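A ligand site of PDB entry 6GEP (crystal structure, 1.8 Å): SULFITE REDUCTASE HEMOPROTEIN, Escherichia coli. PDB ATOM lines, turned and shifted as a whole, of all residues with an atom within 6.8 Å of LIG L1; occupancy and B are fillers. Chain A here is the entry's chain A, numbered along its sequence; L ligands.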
ATOM      1  N   ALA A 360      -5.001 -11.656  11.009  1.00  0.00           N
ATOM      2  CA  ALA A 360      -4.986 -11.780  12.458  1.00  0.00           C
ATOM      3  C   ALA A 360      -3.555 -12.061  12.915  1.00  0.00           C
ATOM      4  O   ALA A 360      -2.735 -12.552  12.132  1.00  0.00           O
ATOM      5  CB  ALA A 360      -5.903 -12.909  12.901  1.00  0.00           C
ATOM      6  N   CYS A 361      -3.237 -11.676  14.151  1.00  0.00           N
ATOM      7  CA  CYS A 361      -1.910 -11.951  14.716  1.00  0.00           C
ATOM      8  C   CYS A 361      -1.906 -13.364  15.329  1.00  0.00           C
ATOM      9  O   CYS A 361      -2.955 -13.999  15.452  1.00  0.00           O
ATOM     10  CB  CYS A 361      -1.568 -10.938  15.816  1.00  0.00           C
ATOM     11  SG  CYS A 361      -2.556 -11.181  17.323  1.00  0.00           S
ATOM     12  N   VAL A 362      -0.723 -13.829  15.721  1.00  0.00           N
ATOM     13  CA  VAL A 362      -0.570 -15.158  16.336  1.00  0.00           C
ATOM     14  C   VAL A 362      -1.437 -15.345  17.594  1.00  0.00           C
ATOM     15  O   VAL A 362      -2.284 -16.240  17.629  1.00  0.00           O
ATOM     16  CB  VAL A 362       0.911 -15.435  16.703  1.00  0.00           C
ATOM     17  CG1 VAL A 362       1.040 -16.763  17.447  1.00  0.00           C
ATOM     18  CG2 VAL A 362       1.769 -15.469  15.433  1.00  0.00           C
ATOM     19  N   SER A 363      -1.249 -14.481  18.591  1.00  0.00           N
ATOM     20  CA  SER A 363      -2.015 -14.565  19.831  1.00  0.00           C
ATOM     21  C   SER A 363      -1.827 -15.930  20.506  1.00  0.00           C
ATOM     22  O   SER A 363      -0.720 -16.484  20.467  1.00  0.00           O
ATOM     23  CB  SER A 363      -3.490 -14.294  19.544  1.00  0.00           C
ATOM     24  OG  SER A 363      -4.203 -14.186  20.766  1.00  0.00           O
ATOM     25  N   PHE A 364      -2.868 -16.471  21.140  1.00  0.00           N
ATOM     26  CA  PHE A 364      -2.777 -17.785  21.794  1.00  0.00           C
ATOM     27  C   PHE A 364      -2.556 -18.827  20.711  1.00  0.00           C
ATOM     28  O   PHE A 364      -3.066 -18.675  19.606  1.00  0.00           O
ATOM     29  CB  PHE A 364      -4.076 -18.115  22.546  1.00  0.00           C
ATOM     30  CG  PHE A 364      -4.393 -17.167  23.658  1.00  0.00           C
ATOM     31  CD1 PHE A 364      -3.569 -17.069  24.769  1.00  0.00           C
ATOM     32  CD2 PHE A 364      -5.531 -16.367  23.598  1.00  0.00           C
ATOM     33  CE1 PHE A 364      -3.856 -16.186  25.800  1.00  0.00           C
ATOM     34  CE2 PHE A 364      -5.840 -15.482  24.629  1.00  0.00           C
ATOM     35  CZ  PHE A 364      -4.998 -15.394  25.730  1.00  0.00           C
ATOM     36  N   CYS A 367       1.537 -16.624  22.285  1.00  0.00           N
ATOM     37  CA  CYS A 367       1.867 -15.285  22.726  1.00  0.00           C
ATOM     38  C   CYS A 367       1.598 -15.037  24.184  1.00  0.00           C
ATOM     39  O   CYS A 367       0.462 -15.135  24.630  1.00  0.00           O
ATOM     40  CB  CYS A 367       1.173 -14.212  21.893  1.00  0.00           C
ATOM     41  SG  CYS A 367       1.806 -12.569  22.310  1.00  0.00           S
ATOM     42  N   PRO A 368       2.621 -14.634  24.929  1.00  0.00           N
ATOM     43  CA  PRO A 368       2.479 -14.372  26.369  1.00  0.00           C
ATOM     44  C   PRO A 368       1.702 -13.096  26.716  1.00  0.00           C
ATOM     45  O   PRO A 368       1.304 -12.904  27.872  1.00  0.00           O
ATOM     46  CB  PRO A 368       3.939 -14.292  26.828  1.00  0.00           C
ATOM     47  CG  PRO A 368       4.635 -13.724  25.639  1.00  0.00           C
ATOM     48  CD  PRO A 368       4.028 -14.520  24.507  1.00  0.00           C
ATOM     49  N   LEU A 369       1.491 -12.234  25.728  1.00  0.00           N
ATOM     50  CA  LEU A 369       0.799 -10.975  25.936  1.00  0.00           C
ATOM     51  C   LEU A 369      -0.659 -10.996  25.438  1.00  0.00           C
ATOM     52  O   LEU A 369      -1.378 -10.003  25.584  1.00  0.00           O
ATOM     53  CB  LEU A 369       1.575  -9.847  25.232  1.00  0.00           C
ATOM     54  CG  LEU A 369       3.093  -9.848  25.421  1.00  0.00           C
ATOM     55  CD1 LEU A 369       3.713  -8.668  24.695  1.00  0.00           C
ATOM     56  CD2 LEU A 369       3.454  -9.802  26.906  1.00  0.00           C
ATOM     57  N   ALA A 370      -1.083 -12.130  24.886  1.00  0.00           N
ATOM     58  CA  ALA A 370      -2.436 -12.266  24.339  1.00  0.00           C
ATOM     59  C   ALA A 370      -3.579 -12.071  25.336  1.00  0.00           C
ATOM     60  O   ALA A 370      -3.528 -12.569  26.464  1.00  0.00           O
ATOM     61  CB  ALA A 370      -2.580 -13.613  23.650  1.00  0.00           C
ATOM     62  N   MET A 371      -4.607 -11.347  24.907  1.00  0.00           N
ATOM     63  CA  MET A 371      -5.768 -11.089  25.724  1.00  0.00           C
ATOM     64  C   MET A 371      -6.979 -11.838  25.164  1.00  0.00           C
ATOM     65  O   MET A 371      -7.815 -12.335  25.921  1.00  0.00           O
ATOM     66  CB  MET A 371      -6.060  -9.597  25.778  1.00  0.00           C
ATOM     67  CG  MET A 371      -4.946  -8.775  26.427  1.00  0.00           C
ATOM     68  SD  MET A 371      -5.346  -7.010  26.381  1.00  0.00           S
ATOM     69  CE  MET A 371      -4.019  -6.258  27.382  1.00  0.00           C
ATOM     70  N   ALA A 372      -7.058 -11.924  23.843  1.00  0.00           N
ATOM     71  CA  ALA A 372      -8.163 -12.621  23.195  1.00  0.00           C
ATOM     72  C   ALA A 372      -7.574 -13.350  21.988  1.00  0.00           C
ATOM     73  O   ALA A 372      -6.493 -13.003  21.524  1.00  0.00           O
ATOM     74  CB  ALA A 372      -9.216 -11.620  22.737  1.00  0.00           C
ATOM     75  N   ALA A 374      -6.885 -14.608  18.220  1.00  0.00           N
ATOM     76  CA  ALA A 374      -6.805 -13.870  16.975  1.00  0.00           C
ATOM     77  C   ALA A 374      -6.689 -14.891  15.851  1.00  0.00           C
ATOM     78  O   ALA A 374      -7.671 -15.192  15.177  1.00  0.00           O
ATOM     79  CB  ALA A 374      -5.624 -12.953  16.995  1.00  0.00           C
ATOM     80  N   VAL A 403      -7.986  -8.667  13.038  1.00  0.00           N
ATOM     81  CA  VAL A 403      -8.164  -8.964  14.434  1.00  0.00           C
ATOM     82  C   VAL A 403      -6.801  -9.014  15.081  1.00  0.00           C
ATOM     83  O   VAL A 403      -5.903  -9.714  14.608  1.00  0.00           O
ATOM     84  CB  VAL A 403      -8.812 -10.344  14.589  1.00  0.00           C
ATOM     85  CG1 VAL A 403      -9.030 -10.664  16.064  1.00  0.00           C
ATOM     86  CG2 VAL A 403     -10.139 -10.387  13.832  1.00  0.00           C
ATOM     87  N   THR A 404      -6.607  -8.250  16.138  1.00  0.00           N
ATOM     88  CA  THR A 404      -5.336  -8.278  16.843  1.00  0.00           C
ATOM     89  C   THR A 404      -5.642  -8.754  18.277  1.00  0.00           C
ATOM     90  O   THR A 404      -6.626  -8.334  18.877  1.00  0.00           O
ATOM     91  CB  THR A 404      -4.620  -6.883  16.740  1.00  0.00           C
ATOM     92  OG1 THR A 404      -3.240  -7.023  17.087  1.00  0.00           O
ATOM     93  CG2 THR A 404      -5.280  -5.806  17.618  1.00  0.00           C
ATOM     94  N   GLY A 405      -4.819  -9.668  18.793  1.00  0.00           N
ATOM     95  CA  GLY A 405      -5.028 -10.253  20.117  1.00  0.00           C
ATOM     96  C   GLY A 405      -4.923  -9.387  21.363  1.00  0.00           C
ATOM     97  O   GLY A 405      -5.382  -9.772  22.435  1.00  0.00           O
ATOM     98  N   CYS A 406      -4.235  -8.258  21.248  1.00  0.00           N
ATOM     99  CA  CYS A 406      -4.091  -7.332  22.355  1.00  0.00           C
ATOM    100  C   CYS A 406      -3.744  -6.002  21.676  1.00  0.00           C
ATOM    101  O   CYS A 406      -3.471  -5.982  20.480  1.00  0.00           O
ATOM    102  CB  CYS A 406      -2.997  -7.797  23.336  1.00  0.00           C
ATOM    103  SG  CYS A 406      -1.274  -7.469  22.879  1.00  0.00           S
ATOM    104  N   PRO A 407      -3.779  -4.897  22.432  1.00  0.00           N
ATOM    105  CA  PRO A 407      -3.483  -3.571  21.883  1.00  0.00           C
ATOM    106  C   PRO A 407      -2.085  -3.306  21.282  1.00  0.00           C
ATOM    107  O   PRO A 407      -1.874  -2.281  20.630  1.00  0.00           O
ATOM    108  CB  PRO A 407      -3.834  -2.637  23.043  1.00  0.00           C
ATOM    109  CG  PRO A 407      -3.523  -3.470  24.223  1.00  0.00           C
ATOM    110  CD  PRO A 407      -4.126  -4.788  23.858  1.00  0.00           C
ATOM    111  N   ASN A 408      -1.131  -4.205  21.509  1.00  0.00           N
ATOM    112  CA  ASN A 408       0.192  -4.058  20.906  1.00  0.00           C
ATOM    113  C   ASN A 408      -0.006  -3.888  19.394  1.00  0.00           C
ATOM    114  O   ASN A 408       0.829  -3.261  18.718  1.00  0.00           O
ATOM    115  CB  ASN A 408       1.073  -5.256  21.230  1.00  0.00           C
ATOM    116  CG  ASN A 408       1.664  -5.166  22.618  1.00  0.00           C
ATOM    117  OD1 ASN A 408       1.736  -4.081  23.185  1.00  0.00           O
ATOM    118  ND2 ASN A 408       2.069  -6.288  23.167  1.00  0.00           N
ATOM    119  N   GLY A 409      -1.079  -4.476  18.878  1.00  0.00           N
ATOM    120  CA  GLY A 409      -1.456  -4.287  17.474  1.00  0.00           C
ATOM    121  C   GLY A 409      -0.765  -4.987  16.328  1.00  0.00           C
ATOM    122  O   GLY A 409      -0.896  -4.520  15.189  1.00  0.00           O
ATOM    123  N   CYS A 410      -0.176  -6.140  16.580  1.00  0.00           N
ATOM    124  CA  CYS A 410       0.533  -6.901  15.554  1.00  0.00           C
ATOM    125  C   CYS A 410      -0.312  -7.293  14.341  1.00  0.00           C
ATOM    126  O   CYS A 410       0.212  -7.436  13.247  1.00  0.00           O
ATOM    127  CB  CYS A 410       1.148  -8.158  16.175  1.00  0.00           C
ATOM    128  SG  CYS A 410       2.066  -7.816  17.709  1.00  0.00           S
ATOM    129  N   GLY A 411      -1.613  -7.484  14.544  1.00  0.00           N
ATOM    130  CA  GLY A 411      -2.480  -7.852  13.441  1.00  0.00           C
ATOM    131  C   GLY A 411      -2.828  -6.667  12.543  1.00  0.00           C
ATOM    132  O   GLY A 411      -3.551  -6.844  11.553  1.00  0.00           O
HETATM  133 FE1  LIG L   1      -1.238 -10.527  19.003  1.00  0.00          FE
HETATM  134 FE2  LIG L   1       0.642 -11.199  20.903  1.00  0.00          FE
HETATM  135 FE3  LIG L   1      -0.755  -8.907  21.238  1.00  0.00          FE
HETATM  136 FE4  LIG L   1       0.994  -9.097  19.148  1.00  0.00          FE
HETATM  137  S1  LIG L   1       1.520  -9.118  21.315  1.00  0.00           S
HETATM  138  S2  LIG L   1      -1.102  -8.217  19.127  1.00  0.00           S
HETATM  139  S3  LIG L   1       0.817 -11.328  18.624  1.00  0.00           S
HETATM  140  S4  LIG L   1      -1.606 -11.033  21.136  1.00  0.00           S
HETATM  141 FE1  LG2 L   2       4.639  -7.923  17.100  1.00  0.00          FE
HETATM  142  C1  LG2 L   2       5.484  -8.246  20.299  1.00  0.00           C
HETATM  143  C2  LG2 L   2       4.058 -11.337  16.874  1.00  0.00           C
HETATM  144  C3  LG2 L   2       4.137  -7.641  13.795  1.00  0.00           C
HETATM  145  C4  LG2 L   2       3.779  -4.660  17.567  1.00  0.00           C
HETATM  146  N1  LG2 L   2       4.788  -9.545  18.373  1.00  0.00           N
HETATM  147  C5  LG2 L   2       5.342  -9.441  19.651  1.00  0.00           C
HETATM  148  C6  LG2 L   2       5.680 -10.816  20.158  1.00  0.00           C
HETATM  149  C7  LG2 L   2       7.142 -11.117  19.704  1.00  0.00           C
HETATM  150  C8  LG2 L   2       5.365 -11.027  21.643  1.00  0.00           C
HETATM  151  C9  LG2 L   2       6.515 -10.850  22.628  1.00  0.00           C
HETATM  152  O1  LG2 L   2       7.002  -9.715  22.801  1.00  0.00           O
HETATM  153  O2  LG2 L   2       6.927 -11.847  23.248  1.00  0.00           O
HETATM  154  C10 LG2 L   2       4.627 -11.617  19.410  1.00  0.00           C
HETATM  155  C11 LG2 L   2       5.042 -13.031  19.188  1.00  0.00           C
HETATM  156  C12 LG2 L   2       3.799 -13.897  19.147  1.00  0.00           C
HETATM  157  C13 LG2 L   2       4.107 -15.349  18.823  1.00  0.00           C
HETATM  158  O3  LG2 L   2       3.964 -16.208  19.707  1.00  0.00           O
HETATM  159  O4  LG2 L   2       4.509 -15.627  17.677  1.00  0.00           O
HETATM  160  C14 LG2 L   2       4.407 -10.829  18.132  1.00  0.00           C
HETATM  161  N2  LG2 L   2       4.267  -9.304  15.588  1.00  0.00           N
HETATM  162  C15 LG2 L   2       4.029 -10.638  15.698  1.00  0.00           C
HETATM  163  C16 LG2 L   2       3.727 -11.221  14.311  1.00  0.00           C
HETATM  164  C17 LG2 L   2       4.310 -12.686  14.220  1.00  0.00           C
HETATM  165  C18 LG2 L   2       2.221 -11.073  14.053  1.00  0.00           C
HETATM  166  C19 LG2 L   2       1.722 -11.961  12.941  1.00  0.00           C
HETATM  167  O5  LG2 L   2       0.770 -12.721  13.195  1.00  0.00           O
HETATM  168  O6  LG2 L   2       2.276 -11.909  11.829  1.00  0.00           O
HETATM  169  C20 LG2 L   2       4.460 -10.182  13.435  1.00  0.00           C
HETATM  170  C21 LG2 L   2       5.937 -10.583  13.482  1.00  0.00           C
HETATM  171  C22 LG2 L   2       6.624  -9.539  12.676  1.00  0.00           C
HETATM  172  C23 LG2 L   2       8.083  -9.842  12.482  1.00  0.00           C
HETATM  173  O7  LG2 L   2       8.376 -10.803  11.751  1.00  0.00           O
HETATM  174  O8  LG2 L   2       8.926  -9.130  13.057  1.00  0.00           O
HETATM  175  C24 LG2 L   2       4.246  -8.928  14.240  1.00  0.00           C
HETATM  176  N3  LG2 L   2       4.032  -6.403  15.881  1.00  0.00           N
HETATM  177  C25 LG2 L   2       3.990  -6.488  14.520  1.00  0.00           C
HETATM  178  C26 LG2 L   2       3.280  -5.267  14.057  1.00  0.00           C
HETATM  179  C27 LG2 L   2       2.842  -5.062  12.623  1.00  0.00           C
HETATM  180  C28 LG2 L   2       3.989  -4.750  11.669  1.00  0.00           C
HETATM  181  O9  LG2 L   2       5.122  -4.532  12.124  1.00  0.00           O
HETATM  182  O10 LG2 L   2       3.765  -4.745  10.446  1.00  0.00           O
HETATM  183  C29 LG2 L   2       3.129  -4.412  15.110  1.00  0.00           C
HETATM  184  C30 LG2 L   2       2.423  -3.105  15.088  1.00  0.00           C
HETATM  185  C31 LG2 L   2       3.229  -1.927  14.515  1.00  0.00           C
HETATM  186  C32 LG2 L   2       4.050  -1.244  15.579  1.00  0.00           C
HETATM  187  O11 LG2 L   2       5.125  -1.747  15.920  1.00  0.00           O
HETATM  188  O12 LG2 L   2       3.619  -0.203  16.099  1.00  0.00           O
HETATM  189  C33 LG2 L   2       3.661  -5.160  16.273  1.00  0.00           C
HETATM  190  N4  LG2 L   2       4.714  -6.615  18.638  1.00  0.00           N
HETATM  191  C34 LG2 L   2       4.294  -5.325  18.640  1.00  0.00           C
HETATM  192  C35 LG2 L   2       4.527  -4.756  20.026  1.00  0.00           C
HETATM  193  C36 LG2 L   2       4.263  -3.346  20.421  1.00  0.00           C
HETATM  194  C37 LG2 L   2       5.508  -2.536  20.131  1.00  0.00           C
HETATM  195  C38 LG2 L   2       5.385  -1.109  20.567  1.00  0.00           C
HETATM  196  O13 LG2 L   2       5.958  -0.243  19.879  1.00  0.00           O
HETATM  197  O14 LG2 L   2       4.740  -0.841  21.600  1.00  0.00           O
HETATM  198  C39 LG2 L   2       5.030  -5.777  20.787  1.00  0.00           C
HETATM  199  C40 LG2 L   2       5.345  -5.821  22.261  1.00  0.00           C
HETATM  200  C41 LG2 L   2       6.696  -5.192  22.481  1.00  0.00           C
HETATM  201  O15 LG2 L   2       7.595  -5.377  21.631  1.00  0.00           O
HETATM  202  O16 LG2 L   2       6.859  -4.515  23.507  1.00  0.00           O
HETATM  203  C42 LG2 L   2       5.188  -6.971  19.882  1.00  0.00           C
HETATM  204  N1  LG3 L   3       6.339  -8.056  16.651  1.00  0.00           N
HETATM  205  O1  LG3 L   3       7.055  -7.146  16.435  1.00  0.00           O
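The backbone NH (N) of Cys 410 sits close to a sulfur (S2) of LIG L1, at 3.4 Å.
SG of Cys 410 binds FE4 of LIG L1 (2.2 Å).
SG of Cys 361 is bound to FE1 of LIG L1 (2.2 Å).
A sulfur (S2) of LIG L1 sits close to the backbone NH (N) of Cys 406 (3.8 Å).
The side-chain sulfur of Cys 406 binds an iron atom (FE3) of LIG L1 (2.2 Å).
SG of Cys 367 binds FE2 of LIG L1.
The side-chain hydroxyl (OG1) of Thr 404 lies close to a sulfur (S2) of LIG L1, 3.2 Å away.
ND2 of Asn 408 lies close to S1 of LIG L1 (3.4 Å).
N of Gly 409 sits close to S2 of LIG L1, at 3.7 Å.
S3 of LIG L1 lies close to N of Ser 363.
The side-chain sulfur (SG) of Cys 410 is bound to an iron atom (FE1) of LG2 L2.
An oxygen (O5) of LG2 L2 sits at hydrogen-bond distance from the backbone NH (N) of Val 362 (3.1 Å).
N of Cys 410 is in hydrogen-bond range of OG1 of Thr 404 (3.2 Å).
The backbone NH (N) of Gly 405 lies close to the side-chain sulfur (SG) of Cys 361 (3.1 Å).
The backbone NH (N) of Cys 361 is in hydrogen-bond range of the backbone carbonyl oxygen (O) of Val 403.
The side-chain sulfur (SG) of Cys 406 sits close to the backbone carbonyl oxygen (O) of Leu 369.
The side-chain sulfur (SG) of Cys 367 sits close to the backbone NH (N) of Leu 369 (3.4 Å).
O of Gly 405 is in hydrogen-bond range of N of Met 371 (3.0 Å).
The backbone carbonyl oxygen (O) of Gly 405 is in hydrogen-bond range of the backbone NH (N) of Ala 372 (3.1 Å).
The side-chain hydroxyl of Ser 363 sits at hydrogen-bond distance from the backbone carbonyl oxygen of Ala 372 (2.7 Å).
N1 of LG3 L3 is bound to FE1 of LG2 L2 (1.8 Å).
Merely in contact with LIG L1: Leu 369 (3.98 Å), Ala 370 (3.5 Å) and Gly 405 (3.7 Å).
Hydrophobic or aromatic side chains that line LIG L1: Leu 369 and Ala 370.
11 residues have an atom within 4 Å of LIG L1: Cys 361, Ser 363, Cys 367, Leu 369, Ala 370, Thr 404, Gly 405, Cys 406, Asn 408, Gly 409 and Cys 410.
Along chain A the residues within 4 Å of LIG L1 span positions 361 to 410.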
